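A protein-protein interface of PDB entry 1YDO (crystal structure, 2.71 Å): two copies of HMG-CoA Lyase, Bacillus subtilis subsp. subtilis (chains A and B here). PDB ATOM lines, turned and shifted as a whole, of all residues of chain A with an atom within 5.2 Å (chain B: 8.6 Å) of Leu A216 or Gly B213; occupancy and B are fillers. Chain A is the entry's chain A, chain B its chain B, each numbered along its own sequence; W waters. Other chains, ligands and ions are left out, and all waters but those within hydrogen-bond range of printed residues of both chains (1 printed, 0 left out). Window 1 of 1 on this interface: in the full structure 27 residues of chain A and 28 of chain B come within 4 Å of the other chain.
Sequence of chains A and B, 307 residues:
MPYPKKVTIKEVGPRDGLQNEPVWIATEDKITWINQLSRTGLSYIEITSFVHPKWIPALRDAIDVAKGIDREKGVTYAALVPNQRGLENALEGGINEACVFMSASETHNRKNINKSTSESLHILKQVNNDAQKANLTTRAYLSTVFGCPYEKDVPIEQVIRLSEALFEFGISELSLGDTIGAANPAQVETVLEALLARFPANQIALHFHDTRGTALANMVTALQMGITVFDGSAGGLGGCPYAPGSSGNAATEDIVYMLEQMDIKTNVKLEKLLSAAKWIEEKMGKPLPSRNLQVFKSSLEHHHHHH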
ATOM      1  N   THR A 214     -18.689  14.226 -32.526  1.00  0.00           N
ATOM      2  CA  THR A 214     -17.567  14.978 -33.068  1.00  0.00           C
ATOM      3  C   THR A 214     -18.017  16.256 -33.724  1.00  0.00           C
ATOM      4  O   THR A 214     -17.214  16.975 -34.302  1.00  0.00           O
ATOM      5  CB  THR A 214     -16.745  14.132 -34.082  1.00  0.00           C
ATOM      6  OG1 THR A 214     -17.623  13.561 -35.050  1.00  0.00           O
ATOM      7  CG2 THR A 214     -16.006  12.996 -33.385  1.00  0.00           C
ATOM      8  N   ALA A 215     -19.307  16.541 -33.596  1.00  0.00           N
ATOM      9  CA  ALA A 215     -19.897  17.734 -34.186  1.00  0.00           C
ATOM     10  C   ALA A 215     -19.173  19.025 -33.863  1.00  0.00           C
ATOM     11  O   ALA A 215     -18.651  19.691 -34.754  1.00  0.00           O
ATOM     12  CB  ALA A 215     -21.341  17.866 -33.760  1.00  0.00           C
ATOM     13  N   LEU A 216     -19.173  19.398 -32.593  1.00  0.00           N
ATOM     14  CA  LEU A 216     -18.529  20.629 -32.194  1.00  0.00           C
ATOM     15  C   LEU A 216     -17.072  20.663 -32.631  1.00  0.00           C
ATOM     16  O   LEU A 216     -16.560  21.713 -33.003  1.00  0.00           O
ATOM     17  CB  LEU A 216     -18.662  20.801 -30.687  1.00  0.00           C
ATOM     18  CG  LEU A 216     -19.842  21.642 -30.193  1.00  0.00           C
ATOM     19  CD1 LEU A 216     -21.127  21.209 -30.829  1.00  0.00           C
ATOM     20  CD2 LEU A 216     -19.917  21.521 -28.695  1.00  0.00           C
ATOM     21  N   ALA A 217     -16.420  19.506 -32.598  1.00  0.00           N
ATOM     22  CA  ALA A 217     -15.025  19.391 -33.010  1.00  0.00           C
ATOM     23  C   ALA A 217     -14.905  19.755 -34.475  1.00  0.00           C
ATOM     24  O   ALA A 217     -14.045  20.532 -34.874  1.00  0.00           O
ATOM     25  CB  ALA A 217     -14.536  17.983 -32.793  1.00  0.00           C
ATOM     26  N   ASN A 218     -15.767  19.177 -35.283  1.00  0.00           N
ATOM     27  CA  ASN A 218     -15.751  19.493 -36.692  1.00  0.00           C
ATOM     28  C   ASN A 218     -16.088  20.958 -36.876  1.00  0.00           C
ATOM     29  O   ASN A 218     -15.592  21.615 -37.779  1.00  0.00           O
ATOM     30  CB  ASN A 218     -16.759  18.627 -37.451  1.00  0.00           C
ATOM     31  CG  ASN A 218     -16.428  17.151 -37.374  1.00  0.00           C
ATOM     32  OD1 ASN A 218     -15.262  16.767 -37.462  1.00  0.00           O
ATOM     33  ND2 ASN A 218     -17.447  16.319 -37.218  1.00  0.00           N
ATOM     34  N   MET A 219     -16.926  21.489 -36.007  1.00  0.00           N
ATOM     35  CA  MET A 219     -17.304  22.881 -36.138  1.00  0.00           C
ATOM     36  C   MET A 219     -16.117  23.811 -35.965  1.00  0.00           C
ATOM     37  O   MET A 219     -16.004  24.814 -36.666  1.00  0.00           O
ATOM     38  CB  MET A 219     -18.345  23.212 -35.111  1.00  0.00           C
ATOM     39  CG  MET A 219     -19.165  24.369 -35.502  1.00  0.00           C
ATOM     40  SD  MET A 219     -20.742  24.221 -34.466  1.00  0.00           S
ATOM     41  CE  MET A 219     -21.489  22.576 -35.215  1.00  0.00           C
ATOM     42  N   VAL A 220     -15.241  23.483 -35.023  1.00  0.00           N
ATOM     43  CA  VAL A 220     -14.080  24.311 -34.791  1.00  0.00           C
ATOM     44  C   VAL A 220     -13.239  24.368 -36.052  1.00  0.00           C
ATOM     45  O   VAL A 220     -12.839  25.446 -36.487  1.00  0.00           O
ATOM     46  CB  VAL A 220     -13.231  23.776 -33.632  1.00  0.00           C
ATOM     47  CG1 VAL A 220     -11.902  24.520 -33.579  1.00  0.00           C
ATOM     48  CG2 VAL A 220     -13.982  23.953 -32.323  1.00  0.00           C
ATOM     49  N   ALA A 250     -26.166  18.308 -33.792  1.00  0.00           N
ATOM     50  CA  ALA A 250     -25.590  18.958 -32.630  1.00  0.00           C
ATOM     51  C   ALA A 250     -26.630  19.814 -31.932  1.00  0.00           C
ATOM     52  O   ALA A 250     -27.427  20.480 -32.574  1.00  0.00           O
ATOM     53  CB  ALA A 250     -24.407  19.815 -33.057  1.00  0.00           C
ATOM     54  N   ASP A 254     -25.594  23.833 -27.253  1.00  0.00           N
ATOM     55  CA  ASP A 254     -24.185  23.480 -27.094  1.00  0.00           C
ATOM     56  C   ASP A 254     -23.350  24.279 -28.083  1.00  0.00           C
ATOM     57  O   ASP A 254     -22.235  24.695 -27.788  1.00  0.00           O
ATOM     58  CB  ASP A 254     -23.991  21.986 -27.351  1.00  0.00           C
ATOM     59  CG  ASP A 254     -24.619  21.129 -26.282  1.00  0.00           C
ATOM     60  OD1 ASP A 254     -24.851  19.926 -26.537  1.00  0.00           O
ATOM     61  OD2 ASP A 254     -24.874  21.661 -25.176  1.00  0.00           O
ATOM     62  N   ILE A 255     -23.912  24.474 -29.266  1.00  0.00           N
ATOM     63  CA  ILE A 255     -23.240  25.215 -30.303  1.00  0.00           C
ATOM     64  C   ILE A 255     -23.173  26.676 -29.915  1.00  0.00           C
ATOM     65  O   ILE A 255     -22.129  27.304 -30.034  1.00  0.00           O
ATOM     66  CB  ILE A 255     -23.974  25.090 -31.631  1.00  0.00           C
ATOM     67  CG1 ILE A 255     -23.943  23.641 -32.079  1.00  0.00           C
ATOM     68  CG2 ILE A 255     -23.351  26.001 -32.652  1.00  0.00           C
ATOM     69  CD1 ILE A 255     -24.611  23.421 -33.381  1.00  0.00           C
ATOM     70  N   MET A 258     -20.585  27.141 -26.731  1.00  0.00           N
ATOM     71  CA  MET A 258     -19.186  27.127 -27.071  1.00  0.00           C
ATOM     72  C   MET A 258     -18.761  28.353 -27.860  1.00  0.00           C
ATOM     73  O   MET A 258     -17.690  28.915 -27.629  1.00  0.00           O
ATOM     74  CB  MET A 258     -18.842  25.879 -27.855  1.00  0.00           C
ATOM     75  CG  MET A 258     -17.376  25.802 -28.150  1.00  0.00           C
ATOM     76  SD  MET A 258     -17.045  24.421 -29.402  1.00  0.00           S
ATOM     77  CE  MET A 258     -17.992  25.165 -30.916  1.00  0.00           C
ATOM     78  N   ARG A 291     -25.876  18.629 -23.746  1.00  0.00           N
ATOM     79  CA  ARG A 291     -25.064  18.704 -22.552  1.00  0.00           C
ATOM     80  C   ARG A 291     -25.441  19.913 -21.716  1.00  0.00           C
ATOM     81  O   ARG A 291     -25.617  19.792 -20.510  1.00  0.00           O
ATOM     82  CB  ARG A 291     -23.583  18.803 -22.894  1.00  0.00           C
ATOM     83  CG  ARG A 291     -23.028  17.659 -23.707  1.00  0.00           C
ATOM     84  CD  ARG A 291     -23.135  16.331 -22.994  1.00  0.00           C
ATOM     85  NE  ARG A 291     -22.375  15.317 -23.709  1.00  0.00           N
ATOM     86  CZ  ARG A 291     -22.416  14.019 -23.431  1.00  0.00           C
ATOM     87  NH1 ARG A 291     -23.193  13.576 -22.447  1.00  0.00           N
ATOM     88  NH2 ARG A 291     -21.678  13.169 -24.137  1.00  0.00           N
ATOM     89  N   ASP B 178      -9.538  20.515 -16.802  1.00  0.00           N
ATOM     90  CA  ASP B 178     -10.680  21.404 -16.868  1.00  0.00           C
ATOM     91  C   ASP B 178     -11.703  20.865 -15.879  1.00  0.00           C
ATOM     92  O   ASP B 178     -12.621  20.130 -16.245  1.00  0.00           O
ATOM     93  CB  ASP B 178     -11.276  21.391 -18.272  1.00  0.00           C
ATOM     94  CG  ASP B 178     -12.405  22.373 -18.425  1.00  0.00           C
ATOM     95  OD1 ASP B 178     -13.101  22.303 -19.458  1.00  0.00           O
ATOM     96  OD2 ASP B 178     -12.579  23.208 -17.508  1.00  0.00           O
ATOM     97  N   ILE B 180     -14.237  22.382 -13.768  1.00  0.00           N
ATOM     98  CA  ILE B 180     -15.625  22.787 -13.992  1.00  0.00           C
ATOM     99  C   ILE B 180     -16.129  22.378 -15.386  1.00  0.00           C
ATOM    100  O   ILE B 180     -17.325  22.138 -15.592  1.00  0.00           O
ATOM    101  CB  ILE B 180     -15.812  24.331 -13.787  1.00  0.00           C
ATOM    102  CG1 ILE B 180     -15.354  25.111 -15.026  1.00  0.00           C
ATOM    103  CG2 ILE B 180     -15.010  24.788 -12.586  1.00  0.00           C
ATOM    104  CD1 ILE B 180     -13.882  24.945 -15.367  1.00  0.00           C
ATOM    105  N   GLY B 181     -15.205  22.280 -16.335  1.00  0.00           N
ATOM    106  CA  GLY B 181     -15.567  21.895 -17.686  1.00  0.00           C
ATOM    107  C   GLY B 181     -16.002  23.073 -18.530  1.00  0.00           C
ATOM    108  O   GLY B 181     -16.820  22.920 -19.435  1.00  0.00           O
ATOM    109  N   ALA B 182     -15.453  24.250 -18.244  1.00  0.00           N
ATOM    110  CA  ALA B 182     -15.819  25.450 -18.988  1.00  0.00           C
ATOM    111  C   ALA B 182     -14.661  26.024 -19.788  1.00  0.00           C
ATOM    112  O   ALA B 182     -14.326  27.199 -19.655  1.00  0.00           O
ATOM    113  CB  ALA B 182     -16.378  26.514 -18.034  1.00  0.00           C
ATOM    114  N   ALA B 183     -14.057  25.192 -20.628  1.00  0.00           N
ATOM    115  CA  ALA B 183     -12.945  25.618 -21.467  1.00  0.00           C
ATOM    116  C   ALA B 183     -13.417  25.578 -22.901  1.00  0.00           C
ATOM    117  O   ALA B 183     -14.229  24.738 -23.259  1.00  0.00           O
ATOM    118  CB  ALA B 183     -11.752  24.678 -21.283  1.00  0.00           C
ATOM    119  N   PRO B 185     -12.093  26.043 -27.213  1.00  0.00           N
ATOM    120  CA  PRO B 185     -10.945  25.953 -28.112  1.00  0.00           C
ATOM    121  C   PRO B 185     -10.123  27.223 -28.133  1.00  0.00           C
ATOM    122  O   PRO B 185      -8.926  27.186 -28.403  1.00  0.00           O
ATOM    123  CB  PRO B 185     -11.589  25.672 -29.452  1.00  0.00           C
ATOM    124  CG  PRO B 185     -12.816  24.898 -29.064  1.00  0.00           C
ATOM    125  CD  PRO B 185     -13.337  25.665 -27.899  1.00  0.00           C
ATOM    126  N   HIS B 209     -13.105  17.880 -19.326  1.00  0.00           N
ATOM    127  CA  HIS B 209     -14.394  17.393 -18.848  1.00  0.00           C
ATOM    128  C   HIS B 209     -15.438  17.926 -19.833  1.00  0.00           C
ATOM    129  O   HIS B 209     -15.544  19.134 -20.003  1.00  0.00           O
ATOM    130  CB  HIS B 209     -14.675  17.937 -17.445  1.00  0.00           C
ATOM    131  CG  HIS B 209     -14.025  17.149 -16.353  1.00  0.00           C
ATOM    132  ND1 HIS B 209     -14.057  17.539 -15.029  1.00  0.00           N
ATOM    133  CD2 HIS B 209     -13.328  15.992 -16.384  1.00  0.00           C
ATOM    134  CE1 HIS B 209     -13.406  16.654 -14.296  1.00  0.00           C
ATOM    135  NE2 HIS B 209     -12.954  15.703 -15.092  1.00  0.00           N
ATOM    136  N   ASP B 210     -16.204  17.073 -20.506  1.00  0.00           N
ATOM    137  CA  ASP B 210     -17.175  17.661 -21.418  1.00  0.00           C
ATOM    138  C   ASP B 210     -18.529  17.853 -20.780  1.00  0.00           C
ATOM    139  O   ASP B 210     -19.551  17.432 -21.298  1.00  0.00           O
ATOM    140  CB  ASP B 210     -17.295  16.891 -22.744  1.00  0.00           C
ATOM    141  CG  ASP B 210     -17.885  15.545 -22.578  1.00  0.00           C
ATOM    142  OD1 ASP B 210     -17.411  14.828 -21.661  1.00  0.00           O
ATOM    143  OD2 ASP B 210     -18.805  15.194 -23.368  1.00  0.00           O
ATOM    144  N   THR B 211     -18.506  18.494 -19.622  1.00  0.00           N
ATOM    145  CA  THR B 211     -19.720  18.819 -18.918  1.00  0.00           C
ATOM    146  C   THR B 211     -20.506  19.724 -19.877  1.00  0.00           C
ATOM    147  O   THR B 211     -21.727  19.742 -19.856  1.00  0.00           O
ATOM    148  CB  THR B 211     -19.408  19.589 -17.657  1.00  0.00           C
ATOM    149  OG1 THR B 211     -18.602  18.777 -16.801  1.00  0.00           O
ATOM    150  CG2 THR B 211     -20.672  19.978 -16.957  1.00  0.00           C
ATOM    151  N   ARG B 212     -19.798  20.474 -20.715  1.00  0.00           N
ATOM    152  CA  ARG B 212     -20.460  21.352 -21.661  1.00  0.00           C
ATOM    153  C   ARG B 212     -20.327  20.790 -23.064  1.00  0.00           C
ATOM    154  O   ARG B 212     -20.619  21.462 -24.054  1.00  0.00           O
ATOM    155  CB  ARG B 212     -19.863  22.760 -21.604  1.00  0.00           C
ATOM    156  CG  ARG B 212     -20.677  23.753 -20.790  1.00  0.00           C
ATOM    157  CD  ARG B 212     -20.857  23.317 -19.348  1.00  0.00           C
ATOM    158  NE  ARG B 212     -21.741  24.228 -18.632  1.00  0.00           N
ATOM    159  CZ  ARG B 212     -21.360  25.388 -18.120  1.00  0.00           C
ATOM    160  NH1 ARG B 212     -20.099  25.780 -18.235  1.00  0.00           N
ATOM    161  NH2 ARG B 212     -22.246  26.158 -17.510  1.00  0.00           N
ATOM    162  N   GLY B 213     -19.863  19.552 -23.141  1.00  0.00           N
ATOM    163  CA  GLY B 213     -19.711  18.899 -24.422  1.00  0.00           C
ATOM    164  C   GLY B 213     -18.742  19.560 -25.367  1.00  0.00           C
ATOM    165  O   GLY B 213     -18.947  19.541 -26.579  1.00  0.00           O
ATOM    166  N   THR B 214     -17.675  20.128 -24.828  1.00  0.00           N
ATOM    167  CA  THR B 214     -16.698  20.789 -25.677  1.00  0.00           C
ATOM    168  C   THR B 214     -15.352  20.120 -25.595  1.00  0.00           C
ATOM    169  O   THR B 214     -14.393  20.603 -26.177  1.00  0.00           O
ATOM    170  CB  THR B 214     -16.545  22.303 -25.306  1.00  0.00           C
ATOM    171  OG1 THR B 214     -16.311  22.444 -23.900  1.00  0.00           O
ATOM    172  CG2 THR B 214     -17.806  23.066 -25.658  1.00  0.00           C
ATOM    173  N   ALA B 215     -15.296  18.991 -24.897  1.00  0.00           N
ATOM    174  CA  ALA B 215     -14.047  18.251 -24.714  1.00  0.00           C
ATOM    175  C   ALA B 215     -13.312  17.935 -25.998  1.00  0.00           C
ATOM    176  O   ALA B 215     -12.184  18.374 -26.197  1.00  0.00           O
ATOM    177  CB  ALA B 215     -14.310  16.964 -23.950  1.00  0.00           C
ATOM    178  N   LEU B 216     -13.946  17.152 -26.856  1.00  0.00           N
ATOM    179  CA  LEU B 216     -13.319  16.769 -28.107  1.00  0.00           C
ATOM    180  C   LEU B 216     -12.896  17.986 -28.900  1.00  0.00           C
ATOM    181  O   LEU B 216     -11.834  17.991 -29.525  1.00  0.00           O
ATOM    182  CB  LEU B 216     -14.253  15.869 -28.926  1.00  0.00           C
ATOM    183  CG  LEU B 216     -14.016  14.368 -28.766  1.00  0.00           C
ATOM    184  CD1 LEU B 216     -13.932  13.988 -27.293  1.00  0.00           C
ATOM    185  CD2 LEU B 216     -15.124  13.616 -29.477  1.00  0.00           C
ATOM    186  N   ALA B 217     -13.717  19.026 -28.852  1.00  0.00           N
ATOM    187  CA  ALA B 217     -13.430  20.263 -29.562  1.00  0.00           C
ATOM    188  C   ALA B 217     -12.143  20.843 -29.016  1.00  0.00           C
ATOM    189  O   ALA B 217     -11.251  21.216 -29.772  1.00  0.00           O
ATOM    190  CB  ALA B 217     -14.562  21.237 -29.370  1.00  0.00           C
ATOM    191  N   ASN B 218     -12.044  20.913 -27.694  1.00  0.00           N
ATOM    192  CA  ASN B 218     -10.836  21.440 -27.088  1.00  0.00           C
ATOM    193  C   ASN B 218      -9.681  20.533 -27.445  1.00  0.00           C
ATOM    194  O   ASN B 218      -8.571  20.982 -27.654  1.00  0.00           O
ATOM    195  CB  ASN B 218     -10.973  21.548 -25.570  1.00  0.00           C
ATOM    196  CG  ASN B 218     -12.050  22.510 -25.160  1.00  0.00           C
ATOM    197  OD1 ASN B 218     -12.184  23.588 -25.731  1.00  0.00           O
ATOM    198  ND2 ASN B 218     -12.820  22.134 -24.155  1.00  0.00           N
ATOM    199  N   VAL B 220      -9.101  18.945 -30.211  1.00  0.00           N
ATOM    200  CA  VAL B 220      -8.600  19.241 -31.544  1.00  0.00           C
ATOM    201  C   VAL B 220      -7.629  20.408 -31.502  1.00  0.00           C
ATOM    202  O   VAL B 220      -6.548  20.337 -32.071  1.00  0.00           O
ATOM    203  CB  VAL B 220      -9.747  19.577 -32.522  1.00  0.00           C
ATOM    204  CG1 VAL B 220      -9.164  20.105 -33.825  1.00  0.00           C
ATOM    205  CG2 VAL B 220     -10.582  18.335 -32.802  1.00  0.00           C
ATOM    206  N   THR B 221      -8.025  21.478 -30.821  1.00  0.00           N
ATOM    207  CA  THR B 221      -7.183  22.663 -30.683  1.00  0.00           C
ATOM    208  C   THR B 221      -5.849  22.249 -30.076  1.00  0.00           C
ATOM    209  O   THR B 221      -4.791  22.664 -30.532  1.00  0.00           O
ATOM    210  CB  THR B 221      -7.851  23.712 -29.776  1.00  0.00           C
ATOM    211  OG1 THR B 221      -9.091  24.113 -30.368  1.00  0.00           O
ATOM    212  CG2 THR B 221      -6.967  24.920 -29.616  1.00  0.00           C
ATOM    213  N   SER B 246     -24.873  15.811 -15.111  1.00  0.00           N
ATOM    214  CA  SER B 246     -24.126  16.097 -16.334  1.00  0.00           C
ATOM    215  C   SER B 246     -22.839  15.275 -16.388  1.00  0.00           C
ATOM    216  O   SER B 246     -22.229  15.003 -15.354  1.00  0.00           O
ATOM    217  CB  SER B 246     -23.790  17.588 -16.417  1.00  0.00           C
ATOM    218  OG  SER B 246     -22.999  17.989 -15.320  1.00  0.00           O
ATOM    219  N   SER B 247     -22.432  14.894 -17.599  1.00  0.00           N
ATOM    220  CA  SER B 247     -21.228  14.088 -17.812  1.00  0.00           C
ATOM    221  C   SER B 247     -19.978  14.740 -17.248  1.00  0.00           C
ATOM    222  O   SER B 247     -19.952  15.947 -17.028  1.00  0.00           O
ATOM    223  CB  SER B 247     -21.041  13.795 -19.307  1.00  0.00           C
ATOM    224  OG  SER B 247     -21.292  14.944 -20.101  1.00  0.00           O
ATOM    225  N   GLY B 248     -18.954  13.925 -17.000  1.00  0.00           N
ATOM    226  CA  GLY B 248     -17.709  14.429 -16.455  1.00  0.00           C
ATOM    227  C   GLY B 248     -16.618  14.506 -17.505  1.00  0.00           C
ATOM    228  O   GLY B 248     -16.632  15.390 -18.360  1.00  0.00           O
ATOM    229  N   ALA B 250     -14.299  13.307 -20.795  1.00  0.00           N
ATOM    230  CA  ALA B 250     -14.613  12.826 -22.123  1.00  0.00           C
ATOM    231  C   ALA B 250     -14.552  11.308 -22.180  1.00  0.00           C
ATOM    232  O   ALA B 250     -13.657  10.686 -21.604  1.00  0.00           O
ATOM    233  CB  ALA B 250     -13.638  13.416 -23.121  1.00  0.00           C
ATOM    234  N   MET B 258     -12.586   9.308 -32.666  1.00  0.00           N
ATOM    235  CA  MET B 258     -12.278  10.474 -33.454  1.00  0.00           C
ATOM    236  C   MET B 258     -10.821  10.505 -33.871  1.00  0.00           C
ATOM    237  O   MET B 258     -10.515  10.853 -34.996  1.00  0.00           O
ATOM    238  CB  MET B 258     -12.605  11.737 -32.681  1.00  0.00           C
ATOM    239  CG  MET B 258     -12.366  12.970 -33.504  1.00  0.00           C
ATOM    240  SD  MET B 258     -12.364  14.586 -32.484  1.00  0.00           S
ATOM    241  CE  MET B 258     -10.918  14.176 -31.279  1.00  0.00           C
ATOM    242  N   ARG B 291     -21.019   8.541 -26.542  1.00  0.00           N
ATOM    243  CA  ARG B 291     -21.765   8.511 -27.789  1.00  0.00           C
ATOM    244  C   ARG B 291     -21.516   7.218 -28.545  1.00  0.00           C
ATOM    245  O   ARG B 291     -22.460   6.561 -28.978  1.00  0.00           O
ATOM    246  CB  ARG B 291     -21.393   9.674 -28.693  1.00  0.00           C
ATOM    247  CG  ARG B 291     -21.624  11.044 -28.107  1.00  0.00           C
ATOM    248  CD  ARG B 291     -23.088  11.319 -27.827  1.00  0.00           C
ATOM    249  NE  ARG B 291     -23.287  12.736 -27.507  1.00  0.00           N
ATOM    250  CZ  ARG B 291     -24.405  13.250 -26.999  1.00  0.00           C
ATOM    251  NH1 ARG B 291     -25.437  12.462 -26.748  1.00  0.00           N
ATOM    252  NH2 ARG B 291     -24.492  14.552 -26.738  1.00  0.00           N
HETATM  253  O   HOH W   1     -19.621  12.962 -22.162  1.00  0.00           O
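The guanidinium group (NE) of Arg A291 lies within salt-bridge range of the side-chain carboxylate (OD2) of Asp B210, at 3.6 Å. The guanidinium group (NH1) of Arg A291 lies within hydrogen-bond range of the side-chain hydroxyl (OG) of Ser B247, at 3.3 Å.
O of Thr A214 lies within hydrogen-bond range of ND2 of Asn A218, at 3.0 Å. The side-chain carboxylate (OD1) of Asp A254 lies within hydrogen-bond range of the backbone NH (N) of Arg A291 (3.2 Å). The backbone carbonyl oxygen of Ala B183 lies within hydrogen-bond range of the side-chain hydroxyl of Thr B214, 3.2 Å away. The backbone carbonyl oxygen (O) of Gly B248 sits at hydrogen-bond distance from the backbone NH (N) of Asp B210, at 2.8 Å. OG1 of Thr B211 sits at hydrogen-bond distance from O of Ser B247 (3.1 Å). The backbone carbonyl oxygen of Thr B214 is in hydrogen-bond range of the side-chain amide nitrogen of Asn B218, 3.0 Å away.
Met B258 touches Thr A214 (CG to CG2, 3.6 Å). CD2 of Leu A216 touches O of Gly B213 (3.1 Å). Ala B217 touches Ala A217 (CA to CA, 3.9 Å). CB of Ala A217 touches CG2 of Val B220, at 3.97 Å. Val A220 touches Pro B185. CB of Met A258 touches CG2 of Thr B214 (3.7 Å). Thr B211 touches Arg A291 (O to CB, 3.7 Å). Arg A291 touches Arg B212. Arg A291 touches Gly B213. NE of Arg B291 touches NH2 of Arg A291, at 3.8 Å.
Of the printed residues of chain B, Thr A214 touches Met B258 (3.6 Å). Of the printed residues of chain B, Leu A216 touches Gly B213 (3.1 Å). Of chain B, only Ala B217 and Val B220 come within 4 Å of Ala A217. Gly B181 touches none of the printed residues of chain A. Gly B213 touches two residues of chain A. Printed residues of chain A within 4 Å of Val B220: Ala A217. Ala B250 touches none of the printed residues of chain A. Printed residues of chain A within 4 Å of Arg B291: Arg A291.
Of the 24 printed residues of chain B, 11 touch a printed residue of chain A. Hydrophobic or aromatic side chains of chain B that line the printed part of chain A: Pro B185, Val B220 and Met B258. Hydrophobic or aromatic side chains of chain A that line the printed part of chain B: Leu A216, Ala A217, Val A220 and Met A258. Among the printed residues, 12 pairs touch across the chains. Among the printed residues, Asp or Glu carboxylates within 4 Å of a Lys or Arg side-chain nitrogen of the other chain: Arg A291 with Asp B210.
Thr A214 touches Met B258, and with the chains exchanged Met A258 touches Thr B214. Ala A217 touches its own counterpart, Ala B217. Ala A217 touches Val B220, but with the chains exchanged Val A220 does not touch Ala B217 (4.1 Å). Arg B291 touches its own counterpart, Arg A291. 9 positions are printed for both chains.
Water W1 lies within hydrogen-bond range of OD2 of Asp B210, NH2 of Arg A291 and OG of Ser B247.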
